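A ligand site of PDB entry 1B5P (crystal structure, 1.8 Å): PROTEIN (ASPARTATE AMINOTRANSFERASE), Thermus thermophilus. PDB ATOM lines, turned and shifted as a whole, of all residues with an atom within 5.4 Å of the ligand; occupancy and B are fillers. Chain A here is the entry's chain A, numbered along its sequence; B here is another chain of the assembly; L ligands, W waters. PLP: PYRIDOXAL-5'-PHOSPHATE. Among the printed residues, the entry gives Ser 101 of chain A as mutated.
NZ of Lys 234 is covalently linked to C4A of the ligand (1.4 Å).
An oxygen (O2P) of the ligand is in hydrogen-bond range of the side-chain hydroxyl (OH) of Tyr 64 of chain B.
A nitrogen (N1) of the ligand is in hydrogen-bond range of the side-chain carboxylate of Asp 203, 2.5 Å away.
The side-chain hydroxyl (OH) of Tyr 206 sits at hydrogen-bond distance from an oxygen (O3) of the ligand (2.7 Å).
O2P of the ligand lies within salt-bridge range of NH1 of Arg 242.
The backbone NH (N) of Gly 100 sits at hydrogen-bond distance from an oxygen (O1P) of the ligand, at 2.8 Å.
ND2 of Asn 175 sits at hydrogen-bond distance from O3 of the ligand (2.9 Å).
The backbone NH (N) of Ser 101 sits at hydrogen-bond distance from an oxygen (O3P) of the ligand (2.9 Å).
OG of Ser 101 lies within hydrogen-bond range of O3P of the ligand (3.3 Å).
NZ of Lys 234 sits at hydrogen-bond distance from OH of Tyr 206 (3.4 Å).
O of Asp 203 is in hydrogen-bond range of ND2 of Asn 171 (2.9 Å).
The side-chain hydroxyl (OH) of Tyr 128 is in hydrogen-bond range of the side-chain carboxylate (OD2) of Asp 203, 2.6 Å away.
OH of Tyr 206 sits at hydrogen-bond distance from ND2 of Asn 175 (3.4 Å).
The side-chain hydroxyl of Tyr 206 sits at hydrogen-bond distance from the side-chain hydroxyl of Tyr 322 (3.0 Å).
The guanidinium group (NH2) of Arg 242 lies within hydrogen-bond range of the side-chain hydroxyl (OG) of Ser 101 (3.3 Å).
The backbone carbonyl oxygen (O) of Arg 242 sits close to the backbone NH (N) of Gly 99 (3.4 Å).
The side-chain hydroxyl (OG) of Ser 101 is in hydrogen-bond range of the side-chain hydroxyl (OG1) of Thr 265 of chain B (3.3 Å).
Residues that only touch the ligand: Gly 99 (3.5 Å), Trp 125 (3.5 Å), Asn 171 (3.5 Å), Ile 205 (3.3 Å) and Ala 233 (3.4 Å).
Hydrophobic or aromatic side chains within 4 Å of the ligand: Trp 125, Ile 205, Tyr 206, Ala 233 and Tyr 64 of chain B.
13 residues have an atom within 4 Å of the ligand: Gly 99, Gly 100, Ser 101, Trp 125, Asn 171, Asn 175, Asp 203, Ile 205, Tyr 206, Ala 233, Lys 234, Arg 242 and Tyr 64 of chain B.
Water W3 lies within hydrogen-bond range of an oxygen (O1P) of the ligand, the backbone carbonyl oxygen of Ile 243 and the backbone NH of Ala 233.
Water W1 lies within hydrogen-bond range of OG1 of Thr 265 of chain B (2.7 Å) and O3P of the ligand (3.3 Å).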
ATOM      1  N   GLY A  39       7.196   8.520   2.142  1.00  0.00           N
ATOM      2  CA  GLY A  39       6.080   8.440   1.222  1.00  0.00           C
ATOM      3  C   GLY A  39       5.045   7.497   1.792  1.00  0.00           C
ATOM      4  O   GLY A  39       4.197   6.982   1.057  1.00  0.00           O
ATOM      5  N   VAL A  98      -1.138  -5.940  -6.681  1.00  0.00           N
ATOM      6  CA  VAL A  98      -0.015  -5.839  -5.739  1.00  0.00           C
ATOM      7  C   VAL A  98       0.355  -4.350  -5.671  1.00  0.00           C
ATOM      8  O   VAL A  98       1.262  -3.877  -6.355  1.00  0.00           O
ATOM      9  CB  VAL A  98       1.181  -6.712  -6.208  1.00  0.00           C
ATOM     10  CG1 VAL A  98       2.355  -6.578  -5.245  1.00  0.00           C
ATOM     11  CG2 VAL A  98       0.744  -8.167  -6.324  1.00  0.00           C
ATOM     12  N   GLY A  99      -0.392  -3.642  -4.837  1.00  0.00           N
ATOM     13  CA  GLY A  99      -0.220  -2.226  -4.654  1.00  0.00           C
ATOM     14  C   GLY A  99      -0.956  -1.485  -5.763  1.00  0.00           C
ATOM     15  O   GLY A  99      -1.356  -2.073  -6.770  1.00  0.00           O
ATOM     16  N   GLY A 100      -1.223  -0.211  -5.516  1.00  0.00           N
ATOM     17  CA  GLY A 100      -1.870   0.605  -6.522  1.00  0.00           C
ATOM     18  C   GLY A 100      -0.852   0.742  -7.629  1.00  0.00           C
ATOM     19  O   GLY A 100      -1.222   1.001  -8.779  1.00  0.00           O
ATOM     20  N   SER A 101       0.429   0.541  -7.330  1.00  0.00           N
ATOM     21  CA  SER A 101       1.422   0.661  -8.369  1.00  0.00           C
ATOM     22  C   SER A 101       1.232  -0.413  -9.430  1.00  0.00           C
ATOM     23  O   SER A 101       1.393  -0.132 -10.624  1.00  0.00           O
ATOM     24  CB  SER A 101       2.849   0.640  -7.816  1.00  0.00           C
ATOM     25  OG  SER A 101       3.197  -0.628  -7.304  1.00  0.00           O
ATOM     26  N   GLN A 102       0.831  -1.618  -9.036  1.00  0.00           N
ATOM     27  CA  GLN A 102       0.630  -2.671 -10.042  1.00  0.00           C
ATOM     28  C   GLN A 102      -0.615  -2.433 -10.872  1.00  0.00           C
ATOM     29  O   GLN A 102      -0.676  -2.828 -12.033  1.00  0.00           O
ATOM     30  CB  GLN A 102       0.579  -4.077  -9.438  1.00  0.00           C
ATOM     31  CG  GLN A 102       0.752  -5.113 -10.548  1.00  0.00           C
ATOM     32  CD  GLN A 102       0.369  -6.519 -10.158  1.00  0.00           C
ATOM     33  OE1 GLN A 102      -0.469  -6.733  -9.298  1.00  0.00           O
ATOM     34  NE2 GLN A 102       0.947  -7.474 -10.851  1.00  0.00           N
ATOM     35  N   LEU A 104      -1.682   0.442 -11.864  1.00  0.00           N
ATOM     36  CA  LEU A 104      -1.250   1.360 -12.899  1.00  0.00           C
ATOM     37  C   LEU A 104      -0.354   0.681 -13.912  1.00  0.00           C
ATOM     38  O   LEU A 104      -0.495   0.894 -15.117  1.00  0.00           O
ATOM     39  CB  LEU A 104      -0.531   2.562 -12.298  1.00  0.00           C
ATOM     40  CG  LEU A 104      -1.460   3.478 -11.500  1.00  0.00           C
ATOM     41  CD1 LEU A 104      -0.641   4.201 -10.459  1.00  0.00           C
ATOM     42  CD2 LEU A 104      -2.185   4.435 -12.433  1.00  0.00           C
ATOM     43  N   TRP A 125       3.865  12.225  -9.721  1.00  0.00           N
ATOM     44  CA  TRP A 125       4.455  11.119  -8.989  1.00  0.00           C
ATOM     45  C   TRP A 125       5.496  10.522  -9.940  1.00  0.00           C
ATOM     46  O   TRP A 125       5.225  10.336 -11.125  1.00  0.00           O
ATOM     47  CB  TRP A 125       3.345  10.110  -8.691  1.00  0.00           C
ATOM     48  CG  TRP A 125       3.709   9.030  -7.775  1.00  0.00           C
ATOM     49  CD1 TRP A 125       4.411   9.137  -6.598  1.00  0.00           C
ATOM     50  CD2 TRP A 125       3.338   7.666  -7.893  1.00  0.00           C
ATOM     51  NE1 TRP A 125       4.493   7.918  -5.991  1.00  0.00           N
ATOM     52  CE2 TRP A 125       3.853   6.989  -6.766  1.00  0.00           C
ATOM     53  CE3 TRP A 125       2.637   6.941  -8.866  1.00  0.00           C
ATOM     54  CZ2 TRP A 125       3.643   5.621  -6.570  1.00  0.00           C
ATOM     55  CZ3 TRP A 125       2.447   5.584  -8.671  1.00  0.00           C
ATOM     56  CH2 TRP A 125       2.948   4.938  -7.529  1.00  0.00           C
ATOM     57  N   TYR A 128       4.700   7.511 -12.814  1.00  0.00           N
ATOM     58  CA  TYR A 128       3.831   7.642 -13.988  1.00  0.00           C
ATOM     59  C   TYR A 128       4.589   7.587 -15.303  1.00  0.00           C
ATOM     60  O   TYR A 128       4.318   6.730 -16.136  1.00  0.00           O
ATOM     61  CB  TYR A 128       2.996   8.942 -13.922  1.00  0.00           C
ATOM     62  CG  TYR A 128       1.936   9.005 -12.849  1.00  0.00           C
ATOM     63  CD1 TYR A 128       1.386   7.848 -12.292  1.00  0.00           C
ATOM     64  CD2 TYR A 128       1.490  10.236 -12.380  1.00  0.00           C
ATOM     65  CE1 TYR A 128       0.403   7.931 -11.300  1.00  0.00           C
ATOM     66  CE2 TYR A 128       0.528  10.328 -11.389  1.00  0.00           C
ATOM     67  CZ  TYR A 128      -0.002   9.188 -10.850  1.00  0.00           C
ATOM     68  OH  TYR A 128      -0.949   9.286  -9.870  1.00  0.00           O
ATOM     69  N   ASN A 171      -4.257  12.865 -10.624  1.00  0.00           N
ATOM     70  CA  ASN A 171      -4.001  12.381  -9.272  1.00  0.00           C
ATOM     71  C   ASN A 171      -4.458  13.394  -8.216  1.00  0.00           C
ATOM     72  O   ASN A 171      -3.758  14.374  -7.965  1.00  0.00           O
ATOM     73  CB  ASN A 171      -2.498  12.075  -9.188  1.00  0.00           C
ATOM     74  CG  ASN A 171      -2.017  11.699  -7.788  1.00  0.00           C
ATOM     75  OD1 ASN A 171      -0.919  12.077  -7.398  1.00  0.00           O
ATOM     76  ND2 ASN A 171      -2.806  10.913  -7.070  1.00  0.00           N
ATOM     77  N   ASN A 175       0.264  13.848  -5.132  1.00  0.00           N
ATOM     78  CA  ASN A 175       1.600  13.546  -4.625  1.00  0.00           C
ATOM     79  C   ASN A 175       2.335  14.059  -5.856  1.00  0.00           C
ATOM     80  O   ASN A 175       2.159  13.497  -6.941  1.00  0.00           O
ATOM     81  CB  ASN A 175       1.807  12.035  -4.434  1.00  0.00           C
ATOM     82  CG  ASN A 175       3.234  11.670  -3.995  1.00  0.00           C
ATOM     83  OD1 ASN A 175       4.115  12.530  -3.935  1.00  0.00           O
ATOM     84  ND2 ASN A 175       3.455  10.395  -3.689  1.00  0.00           N
ATOM     85  N   ASP A 203      -5.993   8.427 -10.163  1.00  0.00           N
ATOM     86  CA  ASP A 203      -5.260   7.877  -9.029  1.00  0.00           C
ATOM     87  C   ASP A 203      -5.784   8.540  -7.765  1.00  0.00           C
ATOM     88  O   ASP A 203      -5.358   9.642  -7.392  1.00  0.00           O
ATOM     89  CB  ASP A 203      -3.750   8.143  -9.202  1.00  0.00           C
ATOM     90  CG  ASP A 203      -2.894   7.382  -8.186  1.00  0.00           C
ATOM     91  OD1 ASP A 203      -3.426   6.826  -7.205  1.00  0.00           O
ATOM     92  OD2 ASP A 203      -1.673   7.325  -8.392  1.00  0.00           O
ATOM     93  N   ILE A 205      -5.591   7.274  -4.478  1.00  0.00           N
ATOM     94  CA  ILE A 205      -5.131   6.654  -3.210  1.00  0.00           C
ATOM     95  C   ILE A 205      -5.199   7.546  -1.976  1.00  0.00           C
ATOM     96  O   ILE A 205      -5.306   7.027  -0.867  1.00  0.00           O
ATOM     97  CB  ILE A 205      -3.676   6.063  -3.225  1.00  0.00           C
ATOM     98  CG1 ILE A 205      -2.856   6.626  -4.351  1.00  0.00           C
ATOM     99  CG2 ILE A 205      -3.680   4.545  -3.081  1.00  0.00           C
ATOM    100  CD1 ILE A 205      -2.484   8.000  -4.068  1.00  0.00           C
ATOM    101  N   TYR A 206      -5.087   8.867  -2.118  1.00  0.00           N
ATOM    102  CA  TYR A 206      -5.110   9.774  -0.961  1.00  0.00           C
ATOM    103  C   TYR A 206      -6.475  10.335  -0.584  1.00  0.00           C
ATOM    104  O   TYR A 206      -6.557  11.217   0.250  1.00  0.00           O
ATOM    105  CB  TYR A 206      -4.154  10.939  -1.160  1.00  0.00           C
ATOM    106  CG  TYR A 206      -2.715  10.552  -1.164  1.00  0.00           C
ATOM    107  CD1 TYR A 206      -2.056  10.240   0.003  1.00  0.00           C
ATOM    108  CD2 TYR A 206      -2.011  10.477  -2.361  1.00  0.00           C
ATOM    109  CE1 TYR A 206      -0.716   9.861   0.004  1.00  0.00           C
ATOM    110  CE2 TYR A 206      -0.690  10.103  -2.390  1.00  0.00           C
ATOM    111  CZ  TYR A 206      -0.045   9.789  -1.204  1.00  0.00           C
ATOM    112  OH  TYR A 206       1.268   9.419  -1.244  1.00  0.00           O
ATOM    113  N   GLY A 231      -6.261   2.006  -3.314  1.00  0.00           N
ATOM    114  CA  GLY A 231      -5.539   1.002  -2.548  1.00  0.00           C
ATOM    115  C   GLY A 231      -5.592   1.267  -1.052  1.00  0.00           C
ATOM    116  O   GLY A 231      -5.984   2.353  -0.618  1.00  0.00           O
ATOM    117  N   ALA A 233      -2.929   1.204   0.936  1.00  0.00           N
ATOM    118  CA  ALA A 233      -1.630   1.709   1.364  1.00  0.00           C
ATOM    119  C   ALA A 233      -1.531   2.958   2.220  1.00  0.00           C
ATOM    120  O   ALA A 233      -0.980   2.917   3.310  1.00  0.00           O
ATOM    121  CB  ALA A 233      -0.714   1.874   0.168  1.00  0.00           C
ATOM    122  N   LYS A 234      -2.104   4.057   1.727  1.00  0.00           N
ATOM    123  CA  LYS A 234      -1.999   5.331   2.410  1.00  0.00           C
ATOM    124  C   LYS A 234      -3.068   5.559   3.464  1.00  0.00           C
ATOM    125  O   LYS A 234      -2.780   6.095   4.536  1.00  0.00           O
ATOM    126  CB  LYS A 234      -1.989   6.429   1.353  1.00  0.00           C
ATOM    127  CG  LYS A 234      -0.998   6.159   0.210  1.00  0.00           C
ATOM    128  CD  LYS A 234       0.473   6.328   0.647  1.00  0.00           C
ATOM    129  CE  LYS A 234       1.460   5.701  -0.349  1.00  0.00           C
ATOM    130  NZ  LYS A 234       1.009   6.028  -1.689  1.00  0.00           N
ATOM    131  N   THR A 239       1.253   0.132   3.503  1.00  0.00           N
ATOM    132  CA  THR A 239       2.186   0.195   2.375  1.00  0.00           C
ATOM    133  C   THR A 239       2.961  -1.100   2.140  1.00  0.00           C
ATOM    134  O   THR A 239       3.131  -1.541   1.007  1.00  0.00           O
ATOM    135  CB  THR A 239       3.202   1.360   2.487  1.00  0.00           C
ATOM    136  OG1 THR A 239       3.891   1.284   3.738  1.00  0.00           O
ATOM    137  CG2 THR A 239       2.503   2.709   2.345  1.00  0.00           C
ATOM    138  N   ARG A 242       1.157  -4.483   0.259  1.00  0.00           N
ATOM    139  CA  ARG A 242       1.023  -4.555  -1.191  1.00  0.00           C
ATOM    140  C   ARG A 242      -0.351  -4.980  -1.734  1.00  0.00           C
ATOM    141  O   ARG A 242      -0.485  -6.011  -2.407  1.00  0.00           O
ATOM    142  CB  ARG A 242       2.138  -5.407  -1.815  1.00  0.00           C
ATOM    143  CG  ARG A 242       3.551  -5.174  -1.240  1.00  0.00           C
ATOM    144  CD  ARG A 242       4.011  -3.720  -1.303  1.00  0.00           C
ATOM    145  NE  ARG A 242       3.858  -3.156  -2.644  1.00  0.00           N
ATOM    146  CZ  ARG A 242       3.182  -2.048  -2.903  1.00  0.00           C
ATOM    147  NH1 ARG A 242       2.577  -1.369  -1.937  1.00  0.00           N
ATOM    148  NH2 ARG A 242       3.043  -1.636  -4.149  1.00  0.00           N
ATOM    149  N   ILE A 243      -1.384  -4.188  -1.406  1.00  0.00           N
ATOM    150  CA  ILE A 243      -2.736  -4.443  -1.877  1.00  0.00           C
ATOM    151  C   ILE A 243      -3.327  -3.156  -2.411  1.00  0.00           C
ATOM    152  O   ILE A 243      -3.481  -2.170  -1.694  1.00  0.00           O
ATOM    153  CB  ILE A 243      -3.688  -4.988  -0.774  1.00  0.00           C
ATOM    154  CG1 ILE A 243      -3.293  -6.407  -0.351  1.00  0.00           C
ATOM    155  CG2 ILE A 243      -5.139  -4.977  -1.275  1.00  0.00           C
ATOM    156  CD1 ILE A 243      -3.395  -7.444  -1.447  1.00  0.00           C
ATOM    157  N   GLY A 244      -3.606  -3.167  -3.705  1.00  0.00           N
ATOM    158  CA  GLY A 244      -4.205  -2.040  -4.382  1.00  0.00           C
ATOM    159  C   GLY A 244      -5.450  -2.536  -5.093  1.00  0.00           C
ATOM    160  O   GLY A 244      -5.726  -3.748  -5.091  1.00  0.00           O
ATOM    161  N   TYR A 322       2.155  15.907   2.071  1.00  0.00           N
ATOM    162  CA  TYR A 322       3.289  16.553   1.414  1.00  0.00           C
ATOM    163  C   TYR A 322       3.107  18.051   1.255  1.00  0.00           C
ATOM    164  O   TYR A 322       1.982  18.551   1.157  1.00  0.00           O
ATOM    165  CB  TYR A 322       3.474  15.998   0.006  1.00  0.00           C
ATOM    166  CG  TYR A 322       3.574  14.505  -0.042  1.00  0.00           C
ATOM    167  CD1 TYR A 322       4.632  13.856   0.573  1.00  0.00           C
ATOM    168  CD2 TYR A 322       2.587  13.742  -0.649  1.00  0.00           C
ATOM    169  CE1 TYR A 322       4.713  12.484   0.581  1.00  0.00           C
ATOM    170  CE2 TYR A 322       2.652  12.359  -0.652  1.00  0.00           C
ATOM    171  CZ  TYR A 322       3.729  11.733  -0.033  1.00  0.00           C
ATOM    172  OH  TYR A 322       3.821  10.368  -0.022  1.00  0.00           O
ATOM    173  N   TYR B  64       7.118  -0.270   3.475  1.00  0.00           N
ATOM    174  CA  TYR B  64       7.744  -0.637   2.208  1.00  0.00           C
ATOM    175  C   TYR B  64       9.137  -1.231   2.426  1.00  0.00           C
ATOM    176  O   TYR B  64       9.900  -0.791   3.298  1.00  0.00           O
ATOM    177  CB  TYR B  64       7.920   0.592   1.311  1.00  0.00           C
ATOM    178  CG  TYR B  64       6.664   1.199   0.710  1.00  0.00           C
ATOM    179  CD1 TYR B  64       5.847   0.473  -0.173  1.00  0.00           C
ATOM    180  CD2 TYR B  64       6.373   2.530   0.914  1.00  0.00           C
ATOM    181  CE1 TYR B  64       4.792   1.085  -0.844  1.00  0.00           C
ATOM    182  CE2 TYR B  64       5.317   3.156   0.249  1.00  0.00           C
ATOM    183  CZ  TYR B  64       4.537   2.438  -0.630  1.00  0.00           C
ATOM    184  OH  TYR B  64       3.543   3.062  -1.334  1.00  0.00           O
ATOM    185  N   THR B 265       6.726  -2.589  -6.783  1.00  0.00           N
ATOM    186  CA  THR B 265       7.550  -1.878  -5.799  1.00  0.00           C
ATOM    187  C   THR B 265       8.425  -2.896  -5.035  1.00  0.00           C
ATOM    188  O   THR B 265       9.638  -2.846  -5.134  1.00  0.00           O
ATOM    189  CB  THR B 265       6.752  -0.935  -4.856  1.00  0.00           C
ATOM    190  OG1 THR B 265       6.006  -0.013  -5.665  1.00  0.00           O
ATOM    191  CG2 THR B 265       7.724  -0.121  -3.990  1.00  0.00           C
HETATM  192  N1  PLP L   1      -0.175   6.815  -6.450  1.00  0.00           N
HETATM  193  C2  PLP L   1       0.420   7.724  -5.621  1.00  0.00           C
HETATM  194  C2A PLP L   1       0.432   9.196  -6.035  1.00  0.00           C
HETATM  195  C3  PLP L   1       0.986   7.315  -4.459  1.00  0.00           C
HETATM  196  O3  PLP L   1       1.574   8.216  -3.646  1.00  0.00           O
HETATM  197  C4  PLP L   1       0.937   5.954  -4.120  1.00  0.00           C
HETATM  198  C4A PLP L   1       1.558   5.531  -2.819  1.00  0.00           C
HETATM  199  C5  PLP L   1       0.310   5.037  -5.004  1.00  0.00           C
HETATM  200  C6  PLP L   1      -0.234   5.499  -6.142  1.00  0.00           C
HETATM  201  C5A PLP L   1       0.209   3.548  -4.782  1.00  0.00           C
HETATM  202  O4P PLP L   1       1.005   2.924  -3.784  1.00  0.00           O
HETATM  203  P   PLP L   1       1.005   1.379  -3.531  1.00  0.00           P
HETATM  204  O1P PLP L   1      -0.359   0.982  -3.139  1.00  0.00           O
HETATM  205  O2P PLP L   1       2.032   1.339  -2.330  1.00  0.00           O
HETATM  206  O3P PLP L   1       1.623   0.736  -4.691  1.00  0.00           O
HETATM  207  O   HOH W   1       4.622   2.050  -4.556  1.00  0.00           O
HETATM  208  O   HOH W   2       4.856   5.089  -3.268  1.00  0.00           O
HETATM  209  O   HOH W   3      -2.297   0.354  -1.731  1.00  0.00           O
